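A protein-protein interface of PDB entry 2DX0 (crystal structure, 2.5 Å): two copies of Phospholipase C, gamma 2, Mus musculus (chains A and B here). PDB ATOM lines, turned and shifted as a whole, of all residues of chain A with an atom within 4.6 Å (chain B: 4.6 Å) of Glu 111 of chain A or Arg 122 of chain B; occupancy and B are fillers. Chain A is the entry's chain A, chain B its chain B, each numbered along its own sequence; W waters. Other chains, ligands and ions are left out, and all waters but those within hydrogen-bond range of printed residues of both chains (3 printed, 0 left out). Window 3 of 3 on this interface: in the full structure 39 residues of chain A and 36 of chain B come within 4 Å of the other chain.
The backbone NH (N) of Thr 124 of chain B sits at hydrogen-bond distance from the backbone carbonyl oxygen (O) of Gly 51 of chain A (2.9 Å).
NH2 of Arg 110 of chain A is in hydrogen-bond range of O of Thr 124 of chain B (2.9 Å).
The backbone NH of Leu 123 of chain B sits at hydrogen-bond distance from the backbone carbonyl oxygen of Tyr 109 of chain A.
O of Glu 111 of chain A lies close to NE of Arg 122 of chain B, at 3.4 Å.
The backbone carbonyl oxygen (O) of Asp 50 of chain A sits at hydrogen-bond distance from the side-chain hydroxyl (OG1) of Thr 124 of chain B (2.9 Å).
OE1 of Gln 107 of chain A is in hydrogen-bond range of NH1 of Arg 110 of chain A (3.2 Å).
Gly 51 of chain A touches Arg 122 of chain B (CA to O, 3.7 Å).
O of Gly 51 of chain A touches CA of Leu 123 of chain B (3.6 Å).
Arg 122 of chain B touches Tyr 109 of chain A.
Arg 110 of chain A touches Arg 122 of chain B.
Arg 110 of chain A touches Leu 123 of chain B (CG to O, 3.3 Å).
Ala 112 of chain A touches Arg 122 of chain B.
His 113 of chain A touches Leu 121 of chain B.
NE of Arg 122 of chain B touches CE1 of His 113 of chain A (3.7 Å).
Of the printed residues of chain B, Asp 50 of chain A touches Thr 124 (2.9 Å).
Gln 107 of chain A touches none of the printed residues of chain B.
His 108 of chain A touches none of the printed residues of chain B.
Of chain B, only Arg 122 comes within 4 Å of Glu 111 of chain A.
Printed residues of chain B within 4 Å of Ala 112 of chain A: Arg 122.
Of the printed residues of chain B, His 113 of chain A touches Leu 121 (3.5 Å) and Arg 122 (3.7 Å).
Of the printed residues of chain A, Leu 121 of chain B touches His 113 (3.5 Å).
Printed residues of chain A within 4 Å of Arg 122 of chain B: Gly 51, Tyr 109, Arg 110, Glu 111, Ala 112 and His 113.
Of the 4 printed residues of chain B, 4 touch a printed residue of chain A.
Hydrophobic or aromatic side chains of chain B that line the printed part of chain A: Leu 123.
Hydrophobic or aromatic side chains of chain A that line the printed part of chain B: His 113.
Among the printed residues, 13 pairs touch across the chains.
Among the printed residues, no Asp or Glu carboxylate lies within 4 Å of a Lys or Arg side-chain nitrogen of the other chain.
No position is printed for both chains.
Of the 13 pairs that touch across the chains among the printed residues, none has its exchanged pair printed and touching as well.
Water W1 bridges NH1 of Arg 122 of chain B (2.6 Å) and ND1 of His 113 of chain A (2.6 Å).
Water W2 bridges O of Leu 123 of chain B and O of Arg 110 of chain A.
Water W3 lies within hydrogen-bond range of the guanidinium group (NH2) of Arg 122 of chain B and the side-chain carboxylate (OE2) of Glu 111 of chain A.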
ATOM      1  N   ASP A  50      11.107  25.068 -10.180  1.00  0.00           N
ATOM      2  CA  ASP A  50      10.617  25.770  -9.011  1.00  0.00           C
ATOM      3  C   ASP A  50       9.792  24.699  -8.303  1.00  0.00           C
ATOM      4  O   ASP A  50       9.185  23.853  -8.958  1.00  0.00           O
ATOM      5  CB  ASP A  50       9.727  26.943  -9.422  1.00  0.00           C
ATOM      6  CG  ASP A  50      10.523  28.128  -9.946  1.00  0.00           C
ATOM      7  OD1 ASP A  50       9.910  29.009 -10.584  1.00  0.00           O
ATOM      8  OD2 ASP A  50      11.751  28.183  -9.711  1.00  0.00           O
ATOM      9  N   GLY A  51       9.773  24.719  -6.977  1.00  0.00           N
ATOM     10  CA  GLY A  51       9.027  23.706  -6.257  1.00  0.00           C
ATOM     11  C   GLY A  51       9.971  22.644  -5.729  1.00  0.00           C
ATOM     12  O   GLY A  51       9.555  21.742  -4.998  1.00  0.00           O
ATOM     13  N   GLN A 107       2.731  14.637  -1.363  1.00  0.00           N
ATOM     14  CA  GLN A 107       2.094  14.254  -2.623  1.00  0.00           C
ATOM     15  C   GLN A 107       0.934  15.200  -2.933  1.00  0.00           C
ATOM     16  O   GLN A 107       0.726  15.588  -4.080  1.00  0.00           O
ATOM     17  CB  GLN A 107       1.585  12.800  -2.581  1.00  0.00           C
ATOM     18  CG  GLN A 107       2.606  11.742  -2.136  1.00  0.00           C
ATOM     19  CD  GLN A 107       4.033  12.041  -2.579  1.00  0.00           C
ATOM     20  OE1 GLN A 107       4.275  12.438  -3.725  1.00  0.00           O
ATOM     21  NE2 GLN A 107       4.994  11.836  -1.670  1.00  0.00           N
ATOM     22  N   HIS A 108       0.179  15.575  -1.908  1.00  0.00           N
ATOM     23  CA  HIS A 108      -0.941  16.491  -2.106  1.00  0.00           C
ATOM     24  C   HIS A 108      -0.481  17.834  -2.670  1.00  0.00           C
ATOM     25  O   HIS A 108      -1.067  18.363  -3.608  1.00  0.00           O
ATOM     26  CB  HIS A 108      -1.665  16.753  -0.798  1.00  0.00           C
ATOM     27  CG  HIS A 108      -2.727  17.798  -0.915  1.00  0.00           C
ATOM     28  ND1 HIS A 108      -3.933  17.564  -1.539  1.00  0.00           N
ATOM     29  CD2 HIS A 108      -2.741  19.101  -0.547  1.00  0.00           C
ATOM     30  CE1 HIS A 108      -4.643  18.678  -1.552  1.00  0.00           C
ATOM     31  NE2 HIS A 108      -3.942  19.625  -0.957  1.00  0.00           N
ATOM     32  N   TYR A 109       0.564  18.394  -2.084  1.00  0.00           N
ATOM     33  CA  TYR A 109       1.057  19.672  -2.548  1.00  0.00           C
ATOM     34  C   TYR A 109       1.898  19.590  -3.818  1.00  0.00           C
ATOM     35  O   TYR A 109       2.490  20.572  -4.262  1.00  0.00           O
ATOM     36  CB  TYR A 109       1.786  20.375  -1.412  1.00  0.00           C
ATOM     37  CG  TYR A 109       0.797  20.868  -0.385  1.00  0.00           C
ATOM     38  CD1 TYR A 109       0.720  20.285   0.882  1.00  0.00           C
ATOM     39  CD2 TYR A 109      -0.123  21.876  -0.710  1.00  0.00           C
ATOM     40  CE1 TYR A 109      -0.245  20.683   1.797  1.00  0.00           C
ATOM     41  CE2 TYR A 109      -1.095  22.282   0.196  1.00  0.00           C
ATOM     42  CZ  TYR A 109      -1.155  21.678   1.449  1.00  0.00           C
ATOM     43  OH  TYR A 109      -2.151  22.035   2.335  1.00  0.00           O
ATOM     44  N   ARG A 110       1.929  18.402  -4.404  1.00  0.00           N
ATOM     45  CA  ARG A 110       2.624  18.192  -5.657  1.00  0.00           C
ATOM     46  C   ARG A 110       1.542  18.269  -6.736  1.00  0.00           C
ATOM     47  O   ARG A 110       1.839  18.353  -7.923  1.00  0.00           O
ATOM     48  CB  ARG A 110       3.311  16.823  -5.675  1.00  0.00           C
ATOM     49  CG  ARG A 110       4.802  16.889  -5.388  1.00  0.00           C
ATOM     50  CD  ARG A 110       5.408  15.525  -5.112  1.00  0.00           C
ATOM     51  NE  ARG A 110       6.854  15.551  -5.306  1.00  0.00           N
ATOM     52  CZ  ARG A 110       7.683  14.569  -4.967  1.00  0.00           C
ATOM     53  NH1 ARG A 110       7.223  13.460  -4.399  1.00  0.00           N
ATOM     54  NH2 ARG A 110       8.980  14.695  -5.209  1.00  0.00           N
ATOM     55  N   GLU A 111       0.283  18.260  -6.296  1.00  0.00           N
ATOM     56  CA  GLU A 111      -0.867  18.327  -7.197  1.00  0.00           C
ATOM     57  C   GLU A 111      -1.719  19.556  -6.950  1.00  0.00           C
ATOM     58  O   GLU A 111      -2.572  19.883  -7.758  1.00  0.00           O
ATOM     59  CB  GLU A 111      -1.763  17.093  -7.041  1.00  0.00           C
ATOM     60  CG  GLU A 111      -1.171  15.784  -7.545  1.00  0.00           C
ATOM     61  CD  GLU A 111      -0.733  15.857  -8.998  1.00  0.00           C
ATOM     62  OE1 GLU A 111       0.425  16.263  -9.253  1.00  0.00           O
ATOM     63  OE2 GLU A 111      -1.548  15.519  -9.889  1.00  0.00           O
ATOM     64  N   ALA A 112      -1.499  20.229  -5.829  1.00  0.00           N
ATOM     65  CA  ALA A 112      -2.281  21.409  -5.490  1.00  0.00           C
ATOM     66  C   ALA A 112      -1.358  22.496  -4.958  1.00  0.00           C
ATOM     67  O   ALA A 112      -0.433  22.217  -4.207  1.00  0.00           O
ATOM     68  CB  ALA A 112      -3.328  21.044  -4.445  1.00  0.00           C
ATOM     69  N   HIS A 113      -1.613  23.739  -5.341  1.00  0.00           N
ATOM     70  CA  HIS A 113      -0.769  24.843  -4.899  1.00  0.00           C
ATOM     71  C   HIS A 113      -0.669  24.905  -3.387  1.00  0.00           C
ATOM     72  O   HIS A 113      -1.629  24.611  -2.683  1.00  0.00           O
ATOM     73  CB  HIS A 113      -1.298  26.183  -5.429  1.00  0.00           C
ATOM     74  CG  HIS A 113      -1.305  26.284  -6.924  1.00  0.00           C
ATOM     75  ND1 HIS A 113      -2.211  25.608  -7.715  1.00  0.00           N
ATOM     76  CD2 HIS A 113      -0.503  26.970  -7.775  1.00  0.00           C
ATOM     77  CE1 HIS A 113      -1.967  25.872  -8.987  1.00  0.00           C
ATOM     78  NE2 HIS A 113      -0.935  26.696  -9.051  1.00  0.00           N
ATOM     79  N   LEU B 121       2.575  27.792  -5.212  1.00  0.00           N
ATOM     80  CA  LEU B 121       2.881  26.937  -6.344  1.00  0.00           C
ATOM     81  C   LEU B 121       2.878  25.487  -5.890  1.00  0.00           C
ATOM     82  O   LEU B 121       2.681  25.194  -4.714  1.00  0.00           O
ATOM     83  CB  LEU B 121       4.258  27.294  -6.915  1.00  0.00           C
ATOM     84  CG  LEU B 121       5.478  26.971  -6.043  1.00  0.00           C
ATOM     85  CD1 LEU B 121       6.749  27.393  -6.757  1.00  0.00           C
ATOM     86  CD2 LEU B 121       5.367  27.691  -4.715  1.00  0.00           C
ATOM     87  N   ARG B 122       3.109  24.581  -6.831  1.00  0.00           N
ATOM     88  CA  ARG B 122       3.130  23.160  -6.529  1.00  0.00           C
ATOM     89  C   ARG B 122       4.545  22.656  -6.307  1.00  0.00           C
ATOM     90  O   ARG B 122       5.469  23.058  -7.005  1.00  0.00           O
ATOM     91  CB  ARG B 122       2.496  22.371  -7.673  1.00  0.00           C
ATOM     92  CG  ARG B 122       1.039  22.715  -7.928  1.00  0.00           C
ATOM     93  CD  ARG B 122       0.468  21.892  -9.071  1.00  0.00           C
ATOM     94  NE  ARG B 122      -0.898  22.299  -9.372  1.00  0.00           N
ATOM     95  CZ  ARG B 122      -1.673  21.726 -10.288  1.00  0.00           C
ATOM     96  NH1 ARG B 122      -2.906  22.180 -10.483  1.00  0.00           N
ATOM     97  NH2 ARG B 122      -1.219  20.701 -11.009  1.00  0.00           N
ATOM     98  N   LEU B 123       4.710  21.777  -5.324  1.00  0.00           N
ATOM     99  CA  LEU B 123       6.016  21.202  -5.046  1.00  0.00           C
ATOM    100  C   LEU B 123       6.388  20.300  -6.229  1.00  0.00           C
ATOM    101  O   LEU B 123       5.507  19.738  -6.884  1.00  0.00           O
ATOM    102  CB  LEU B 123       5.969  20.376  -3.758  1.00  0.00           C
ATOM    103  CG  LEU B 123       5.690  21.122  -2.451  1.00  0.00           C
ATOM    104  CD1 LEU B 123       5.786  20.129  -1.296  1.00  0.00           C
ATOM    105  CD2 LEU B 123       6.701  22.282  -2.260  1.00  0.00           C
ATOM    106  N   THR B 124       7.681  20.172  -6.511  1.00  0.00           N
ATOM    107  CA  THR B 124       8.109  19.321  -7.619  1.00  0.00           C
ATOM    108  C   THR B 124       9.162  18.282  -7.249  1.00  0.00           C
ATOM    109  O   THR B 124       8.862  17.264  -6.625  1.00  0.00           O
ATOM    110  CB  THR B 124       8.649  20.156  -8.832  1.00  0.00           C
ATOM    111  OG1 THR B 124       9.681  21.047  -8.393  1.00  0.00           O
ATOM    112  CG2 THR B 124       7.510  20.967  -9.487  1.00  0.00           C
HETATM  113  O   HOH W   1      -3.655  23.609  -8.487  1.00  0.00           O
HETATM  114  O   HOH W   2       4.216  19.225  -9.077  1.00  0.00           O
HETATM  115  O   HOH W   3      -2.965  18.148 -11.173  1.00  0.00           O
